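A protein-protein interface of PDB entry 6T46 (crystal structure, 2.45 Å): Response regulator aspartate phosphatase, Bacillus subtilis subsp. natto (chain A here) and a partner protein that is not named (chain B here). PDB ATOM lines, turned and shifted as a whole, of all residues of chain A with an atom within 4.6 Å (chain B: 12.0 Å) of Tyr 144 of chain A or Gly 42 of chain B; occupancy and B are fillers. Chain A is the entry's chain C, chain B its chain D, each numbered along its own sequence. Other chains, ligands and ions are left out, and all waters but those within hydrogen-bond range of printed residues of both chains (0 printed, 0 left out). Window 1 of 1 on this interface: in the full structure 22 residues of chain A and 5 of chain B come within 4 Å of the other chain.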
ATOM      1  N   GLY A 140     -15.146  14.636 -16.144  1.00  0.00           N
ATOM      2  CA  GLY A 140     -14.859  13.609 -15.157  1.00  0.00           C
ATOM      3  C   GLY A 140     -16.107  12.907 -14.651  1.00  0.00           C
ATOM      4  O   GLY A 140     -16.152  11.667 -14.582  1.00  0.00           O
ATOM      5  N   VAL A 141     -17.170  13.663 -14.352  1.00  0.00           N
ATOM      6  CA  VAL A 141     -18.389  12.976 -13.911  1.00  0.00           C
ATOM      7  C   VAL A 141     -18.916  12.090 -15.035  1.00  0.00           C
ATOM      8  O   VAL A 141     -19.385  10.975 -14.801  1.00  0.00           O
ATOM      9  CB  VAL A 141     -19.486  13.972 -13.474  1.00  0.00           C
ATOM     10  CG1 VAL A 141     -20.856  13.248 -13.418  1.00  0.00           C
ATOM     11  CG2 VAL A 141     -19.161  14.670 -12.152  1.00  0.00           C
ATOM     12  N   ALA A 142     -18.862  12.579 -16.277  1.00  0.00           N
ATOM     13  CA  ALA A 142     -19.368  11.781 -17.385  1.00  0.00           C
ATOM     14  C   ALA A 142     -18.573  10.488 -17.542  1.00  0.00           C
ATOM     15  O   ALA A 142     -19.162   9.423 -17.727  1.00  0.00           O
ATOM     16  CB  ALA A 142     -19.346  12.604 -18.670  1.00  0.00           C
ATOM     17  N   TYR A 143     -17.243  10.541 -17.423  1.00  0.00           N
ATOM     18  CA  TYR A 143     -16.477   9.295 -17.490  1.00  0.00           C
ATOM     19  C   TYR A 143     -16.882   8.355 -16.370  1.00  0.00           C
ATOM     20  O   TYR A 143     -17.090   7.148 -16.586  1.00  0.00           O
ATOM     21  CB  TYR A 143     -14.980   9.567 -17.369  1.00  0.00           C
ATOM     22  CG  TYR A 143     -14.304   9.951 -18.660  1.00  0.00           C
ATOM     23  CD1 TYR A 143     -14.357   9.132 -19.784  1.00  0.00           C
ATOM     24  CD2 TYR A 143     -13.575  11.115 -18.738  1.00  0.00           C
ATOM     25  CE1 TYR A 143     -13.726   9.500 -20.959  1.00  0.00           C
ATOM     26  CE2 TYR A 143     -12.942  11.476 -19.885  1.00  0.00           C
ATOM     27  CZ  TYR A 143     -13.019  10.664 -20.988  1.00  0.00           C
ATOM     28  OH  TYR A 143     -12.368  11.072 -22.119  1.00  0.00           O
ATOM     29  N   TYR A 144     -17.076   8.909 -15.175  1.00  0.00           N
ATOM     30  CA  TYR A 144     -17.488   8.084 -14.047  1.00  0.00           C
ATOM     31  C   TYR A 144     -18.811   7.398 -14.332  1.00  0.00           C
ATOM     32  O   TYR A 144     -19.027   6.249 -13.919  1.00  0.00           O
ATOM     33  CB  TYR A 144     -17.602   8.950 -12.807  1.00  0.00           C
ATOM     34  CG  TYR A 144     -18.391   8.304 -11.739  1.00  0.00           C
ATOM     35  CD1 TYR A 144     -17.796   7.368 -10.918  1.00  0.00           C
ATOM     36  CD2 TYR A 144     -19.725   8.615 -11.534  1.00  0.00           C
ATOM     37  CE1 TYR A 144     -18.494   6.747  -9.914  1.00  0.00           C
ATOM     38  CE2 TYR A 144     -20.458   7.979 -10.525  1.00  0.00           C
ATOM     39  CZ  TYR A 144     -19.818   7.037  -9.720  1.00  0.00           C
ATOM     40  OH  TYR A 144     -20.466   6.365  -8.697  1.00  0.00           O
ATOM     41  N   GLU A 145     -19.732   8.083 -15.010  1.00  0.00           N
ATOM     42  CA  GLU A 145     -21.012   7.430 -15.246  1.00  0.00           C
ATOM     43  C   GLU A 145     -20.851   6.231 -16.166  1.00  0.00           C
ATOM     44  O   GLU A 145     -21.652   5.295 -16.100  1.00  0.00           O
ATOM     45  CB  GLU A 145     -22.044   8.406 -15.801  1.00  0.00           C
ATOM     46  CG  GLU A 145     -22.417   9.445 -14.761  1.00  0.00           C
ATOM     47  CD  GLU A 145     -23.134   8.861 -13.555  1.00  0.00           C
ATOM     48  OE1 GLU A 145     -23.465   7.654 -13.591  1.00  0.00           O
ATOM     49  OE2 GLU A 145     -23.338   9.597 -12.555  1.00  0.00           O
ATOM     50  N   ILE A 146     -19.850   6.232 -17.035  1.00  0.00           N
ATOM     51  CA  ILE A 146     -19.591   5.071 -17.861  1.00  0.00           C
ATOM     52  C   ILE A 146     -18.407   4.274 -17.329  1.00  0.00           C
ATOM     53  O   ILE A 146     -17.754   3.560 -18.092  1.00  0.00           O
ATOM     54  CB  ILE A 146     -19.399   5.438 -19.331  1.00  0.00           C
ATOM     55  CG1 ILE A 146     -18.299   6.459 -19.432  1.00  0.00           C
ATOM     56  CG2 ILE A 146     -20.697   5.988 -19.872  1.00  0.00           C
ATOM     57  CD1 ILE A 146     -17.919   6.749 -20.820  1.00  0.00           C
ATOM     58  N   ASP A 147     -18.052   4.481 -16.063  1.00  0.00           N
ATOM     59  CA  ASP A 147     -17.141   3.600 -15.327  1.00  0.00           C
ATOM     60  C   ASP A 147     -15.718   3.604 -15.892  1.00  0.00           C
ATOM     61  O   ASP A 147     -15.003   2.607 -15.815  1.00  0.00           O
ATOM     62  CB  ASP A 147     -17.722   2.198 -15.289  1.00  0.00           C
ATOM     63  CG  ASP A 147     -19.072   2.189 -14.600  1.00  0.00           C
ATOM     64  OD1 ASP A 147     -20.078   2.318 -15.333  1.00  0.00           O
ATOM     65  OD2 ASP A 147     -19.140   2.131 -13.341  1.00  0.00           O
ATOM     66  N   HIS A 149     -12.961   5.003 -14.598  1.00  0.00           N
ATOM     67  CA  HIS A 149     -12.593   5.618 -13.319  1.00  0.00           C
ATOM     68  C   HIS A 149     -11.221   6.272 -13.363  1.00  0.00           C
ATOM     69  O   HIS A 149     -11.022   7.354 -12.782  1.00  0.00           O
ATOM     70  CB  HIS A 149     -12.639   4.577 -12.224  1.00  0.00           C
ATOM     71  CG  HIS A 149     -13.966   3.903 -12.129  1.00  0.00           C
ATOM     72  ND1 HIS A 149     -15.111   4.581 -11.781  1.00  0.00           N
ATOM     73  CD2 HIS A 149     -14.350   2.634 -12.409  1.00  0.00           C
ATOM     74  CE1 HIS A 149     -16.142   3.751 -11.808  1.00  0.00           C
ATOM     75  NE2 HIS A 149     -15.710   2.562 -12.198  1.00  0.00           N
ATOM     76  N   SER A 152     -11.568   9.524 -14.942  1.00  0.00           N
ATOM     77  CA  SER A 152     -12.505  10.315 -14.159  1.00  0.00           C
ATOM     78  C   SER A 152     -11.773  10.991 -13.021  1.00  0.00           C
ATOM     79  O   SER A 152     -11.863  12.209 -12.838  1.00  0.00           O
ATOM     80  CB  SER A 152     -13.626   9.433 -13.642  1.00  0.00           C
ATOM     81  OG  SER A 152     -14.623  10.232 -13.024  1.00  0.00           O
ATOM     82  N   ILE A 182     -16.068   8.578  -4.826  1.00  0.00           N
ATOM     83  CA  ILE A 182     -16.889   7.456  -5.271  1.00  0.00           C
ATOM     84  C   ILE A 182     -16.169   6.639  -6.347  1.00  0.00           C
ATOM     85  O   ILE A 182     -16.405   5.428  -6.470  1.00  0.00           O
ATOM     86  CB  ILE A 182     -18.290   7.915  -5.729  1.00  0.00           C
ATOM     87  CG1 ILE A 182     -18.234   8.964  -6.830  1.00  0.00           C
ATOM     88  CG2 ILE A 182     -19.094   8.473  -4.577  1.00  0.00           C
ATOM     89  CD1 ILE A 182     -19.635   9.274  -7.385  1.00  0.00           C
ATOM     90  N   ASN A 183     -15.267   7.263  -7.112  1.00  0.00           N
ATOM     91  CA  ASN A 183     -14.436   6.532  -8.062  1.00  0.00           C
ATOM     92  C   ASN A 183     -13.585   5.492  -7.355  1.00  0.00           C
ATOM     93  O   ASN A 183     -13.511   4.336  -7.792  1.00  0.00           O
ATOM     94  CB  ASN A 183     -13.525   7.484  -8.813  1.00  0.00           C
ATOM     95  CG  ASN A 183     -14.146   7.982 -10.100  1.00  0.00           C
ATOM     96  OD1 ASN A 183     -14.329   9.190 -10.296  1.00  0.00           O
ATOM     97  ND2 ASN A 183     -14.538   7.058 -10.955  1.00  0.00           N
ATOM     98  N   TYR A 185     -14.132   4.097  -4.558  1.00  0.00           N
ATOM     99  CA  TYR A 185     -15.015   3.041  -4.093  1.00  0.00           C
ATOM    100  C   TYR A 185     -15.371   2.121  -5.237  1.00  0.00           C
ATOM    101  O   TYR A 185     -15.284   0.891  -5.113  1.00  0.00           O
ATOM    102  CB  TYR A 185     -16.276   3.661  -3.500  1.00  0.00           C
ATOM    103  CG  TYR A 185     -17.490   2.771  -3.545  1.00  0.00           C
ATOM    104  CD1 TYR A 185     -17.650   1.759  -2.609  1.00  0.00           C
ATOM    105  CD2 TYR A 185     -18.500   2.955  -4.500  1.00  0.00           C
ATOM    106  CE1 TYR A 185     -18.772   0.942  -2.626  1.00  0.00           C
ATOM    107  CE2 TYR A 185     -19.635   2.140  -4.519  1.00  0.00           C
ATOM    108  CZ  TYR A 185     -19.761   1.132  -3.583  1.00  0.00           C
ATOM    109  OH  TYR A 185     -20.871   0.289  -3.579  1.00  0.00           O
ATOM    110  N   ASP A 186     -15.759   2.700  -6.376  1.00  0.00           N
ATOM    111  CA  ASP A 186     -16.071   1.865  -7.529  1.00  0.00           C
ATOM    112  C   ASP A 186     -14.841   1.168  -8.082  1.00  0.00           C
ATOM    113  O   ASP A 186     -14.955   0.037  -8.559  1.00  0.00           O
ATOM    114  CB  ASP A 186     -16.812   2.660  -8.588  1.00  0.00           C
ATOM    115  CG  ASP A 186     -18.299   2.660  -8.328  1.00  0.00           C
ATOM    116  OD1 ASP A 186     -18.856   1.532  -8.257  1.00  0.00           O
ATOM    117  OD2 ASP A 186     -18.906   3.749  -8.137  1.00  0.00           O
ATOM    118  N   ASN A 219     -21.721   7.455   1.350  1.00  0.00           N
ATOM    119  CA  ASN A 219     -20.607   6.836   0.636  1.00  0.00           C
ATOM    120  C   ASN A 219     -19.711   6.076   1.596  1.00  0.00           C
ATOM    121  O   ASN A 219     -19.162   5.025   1.243  1.00  0.00           O
ATOM    122  CB  ASN A 219     -19.806   7.887  -0.125  1.00  0.00           C
ATOM    123  CG  ASN A 219     -20.605   8.514  -1.276  1.00  0.00           C
ATOM    124  OD1 ASN A 219     -21.471   7.867  -1.888  1.00  0.00           O
ATOM    125  ND2 ASN A 219     -20.343   9.796  -1.546  1.00  0.00           N
ATOM    126  N   LEU A 222     -21.420   2.839   1.921  1.00  0.00           N
ATOM    127  CA  LEU A 222     -21.183   1.941   0.794  1.00  0.00           C
ATOM    128  C   LEU A 222     -19.816   1.306   0.888  1.00  0.00           C
ATOM    129  O   LEU A 222     -19.661   0.118   0.581  1.00  0.00           O
ATOM    130  CB  LEU A 222     -21.310   2.684  -0.542  1.00  0.00           C
ATOM    131  CG  LEU A 222     -22.729   3.138  -0.888  1.00  0.00           C
ATOM    132  CD1 LEU A 222     -22.768   3.823  -2.225  1.00  0.00           C
ATOM    133  CD2 LEU A 222     -23.682   1.945  -0.867  1.00  0.00           C
ATOM    134  N   GLN A 254     -31.603   6.010  -2.409  1.00  0.00           N
ATOM    135  CA  GLN A 254     -30.371   5.247  -2.256  1.00  0.00           C
ATOM    136  C   GLN A 254     -30.171   4.825  -0.811  1.00  0.00           C
ATOM    137  O   GLN A 254     -29.827   3.668  -0.535  1.00  0.00           O
ATOM    138  CB  GLN A 254     -29.176   6.069  -2.722  1.00  0.00           C
ATOM    139  CG  GLN A 254     -29.352   6.789  -4.042  1.00  0.00           C
ATOM    140  CD  GLN A 254     -28.062   7.467  -4.431  1.00  0.00           C
ATOM    141  OE1 GLN A 254     -26.984   6.974  -4.084  1.00  0.00           O
ATOM    142  NE2 GLN A 254     -28.147   8.593  -5.130  1.00  0.00           N
ATOM    143  N   GLN B  40     -23.566  -1.194  -5.820  1.00  0.00           N
ATOM    144  CA  GLN B  40     -24.338   0.045  -5.773  1.00  0.00           C
ATOM    145  C   GLN B  40     -23.417   1.239  -5.966  1.00  0.00           C
ATOM    146  O   GLN B  40     -22.522   1.466  -5.144  1.00  0.00           O
ATOM    147  CB  GLN B  40     -25.075   0.166  -4.443  1.00  0.00           C
ATOM    148  CG  GLN B  40     -25.836   1.470  -4.255  1.00  0.00           C
ATOM    149  CD  GLN B  40     -27.218   1.459  -4.893  1.00  0.00           C
ATOM    150  OE1 GLN B  40     -27.623   0.482  -5.540  1.00  0.00           O
ATOM    151  NE2 GLN B  40     -27.963   2.547  -4.690  1.00  0.00           N
ATOM    152  N   LYS B  41     -23.633   2.020  -7.022  1.00  0.00           N
ATOM    153  CA  LYS B  41     -22.786   3.187  -7.201  1.00  0.00           C
ATOM    154  C   LYS B  41     -23.129   4.267  -6.182  1.00  0.00           C
ATOM    155  O   LYS B  41     -24.256   4.353  -5.684  1.00  0.00           O
ATOM    156  CB  LYS B  41     -22.902   3.720  -8.622  1.00  0.00           C
ATOM    157  CG  LYS B  41     -22.612   2.648  -9.634  1.00  0.00           C
ATOM    158  CD  LYS B  41     -22.399   3.221 -11.009  1.00  0.00           C
ATOM    159  CE  LYS B  41     -20.956   3.584 -11.239  1.00  0.00           C
ATOM    160  NZ  LYS B  41     -20.905   4.395 -12.490  1.00  0.00           N
ATOM    161  N   GLY B  42     -22.115   5.060  -5.838  1.00  0.00           N
ATOM    162  CA  GLY B  42     -22.238   6.069  -4.802  1.00  0.00           C
ATOM    163  C   GLY B  42     -23.047   7.273  -5.225  1.00  0.00           C
ATOM    164  O   GLY B  42     -23.426   7.431  -6.389  1.00  0.00           O
ATOM    165  N   MET B  43     -23.341   8.134  -4.251  1.00  0.00           N
ATOM    166  CA  MET B  43     -24.084   9.348  -4.546  1.00  0.00           C
ATOM    167  C   MET B  43     -23.170  10.568  -4.466  1.00  0.00           C
ATOM    168  O   MET B  43     -22.181  10.594  -3.721  1.00  0.00           O
ATOM    169  CB  MET B  43     -25.306   9.517  -3.625  1.00  0.00           C
ATOM    170  CG  MET B  43     -25.031  10.073  -2.239  1.00  0.00           C
ATOM    171  SD  MET B  43     -26.533  10.770  -1.488  1.00  0.00           S
ATOM    172  CE  MET B  43     -27.454   9.266  -1.149  1.00  0.00           C
ATOM    173  N   TYR B  44     -23.479  11.552  -5.292  1.00  0.00           N
ATOM    174  CA  TYR B  44     -22.748  12.801  -5.296  1.00  0.00           C
ATOM    175  C   TYR B  44     -23.767  13.910  -5.615  1.00  0.00           C
ATOM    176  O   TYR B  44     -23.459  15.093  -5.822  1.00  0.00           O
ATOM    177  CB  TYR B  44     -21.598  12.765  -6.302  1.00  0.00           C
ATOM    178  CG  TYR B  44     -22.037  12.517  -7.713  1.00  0.00           C
ATOM    179  CD1 TYR B  44     -22.414  11.256  -8.141  1.00  0.00           C
ATOM    180  CD2 TYR B  44     -22.098  13.547  -8.617  1.00  0.00           C
ATOM    181  CE1 TYR B  44     -22.829  11.042  -9.439  1.00  0.00           C
ATOM    182  CE2 TYR B  44     -22.504  13.341  -9.904  1.00  0.00           C
ATOM    183  CZ  TYR B  44     -22.865  12.091 -10.306  1.00  0.00           C
ATOM    184  OH  TYR B  44     -23.257  11.895 -11.599  1.00  0.00           O
ATOM    185  OXT TYR B  44     -24.982  13.636  -5.659  1.00  0.00           O
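The backbone carbonyl oxygen (O) of Tyr 144 of chain A sits at hydrogen-bond distance from the side-chain amino group (NZ) of Lys 41 of chain B (3.0 Å). The side-chain hydroxyl (OH) of Tyr 44 of chain B sits at hydrogen-bond distance from the side-chain carboxylate (OE2) of Glu 145 of chain A. NZ of Lys 41 of chain B lies within salt-bridge range of OD2 of Asp 147 of chain A. OH of Tyr 185 of chain A lies within hydrogen-bond range of O of Gln 40 of chain B (2.6 Å). The backbone carbonyl oxygen (O) of Met 43 of chain B sits at hydrogen-bond distance from the side-chain amide nitrogen (ND2) of Asn 219 of chain A, 3.0 Å away.
The side-chain hydroxyl (OH) of Tyr 144 of chain A lies within hydrogen-bond range of the side-chain carboxylate (OD2) of Asp 186 of chain A (3.1 Å).
Among the printed residues, merely in contact across the chains: Val 141 of chain A with Tyr 44 of chain B, Tyr 144 of chain A with Gly 42 of chain B, Glu 145 of chain A with Lys 41 of chain B, Ile 182 of chain A with Gly 42 of chain B, Ile 182 of chain A with Met 43 of chain B, Ile 182 of chain A with Tyr 44 of chain B, Asp 186 of chain A with Lys 41 of chain B, Asn 219 of chain A with Gly 42 of chain B, Leu 222 of chain A with Gln 40 of chain B, Leu 222 of chain A with Lys 41 of chain B, Leu 222 of chain A with Gly 42 of chain B and Gln 254 of chain A with Met 43 of chain B.
No residue of chain B comes within 4 Å of Gly 140 of chain A. Of the printed residues of chain B, Val 141 of chain A touches Tyr 44. No residue of chain B comes within 4 Å of Ala 142 of chain A. Tyr 143 of chain A touches none of the printed residues of chain B. Of chain B, only Lys 41 (3.0 Å) and Gly 42 (3.5 Å) come within 4 Å of Tyr 144 of chain A. Of chain B, only Lys 41 and Tyr 44 come within 4 Å of Glu 145 of chain A. Of chain B, only Lys 41 (3.0 Å) comes within 4 Å of Asp 147 of chain A. No residue of chain B comes within 4 Å of Ser 152 of chain A. Of chain B, only Gly 42 (3.96 Å), Met 43 (3.8 Å) and Tyr 44 (3.5 Å) come within 4 Å of Ile 182 of chain A. Of the printed residues of chain B, Tyr 185 of chain A touches Gln 40. Of chain B, only Lys 41 (3.7 Å) comes within 4 Å of Asp 186 of chain A. Of chain B, only Gly 42 (3.5 Å) and Met 43 (3.0 Å) come within 4 Å of Asn 219 of chain A. Of the printed residues of chain B, Gln 254 of chain A touches Met 43 (3.1 Å). Printed residues of chain A within 4 Å of Lys 41 of chain B: Tyr 144 (3.0 Å), Glu 145 (3.8 Å), Asp 147 (3.0 Å), Asp 186 (3.7 Å) and Leu 222 (3.8 Å). Of chain A, only Tyr 144 (3.5 Å), Ile 182 (3.96 Å), Asn 219 (3.5 Å) and Leu 222 (3.5 Å) come within 4 Å of Gly 42 of chain B. The nearest residue of chain B that does not touch Tyr 144 of chain A is Tyr 44 of chain B (4.02 Å).
Hydrophobic or aromatic side chains of chain B within 4 Å of the printed part of chain A: Met 43 and Tyr 44. Of the 17 printed residues of chain A, 10 touch a printed residue of chain B. Hydrophobic or aromatic side chains of chain A within 4 Å of the printed part of chain B: Val 141, Tyr 144, Ile 182, Tyr 185 and Leu 222. Among the printed residues, 17 pairs touch across the chains.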
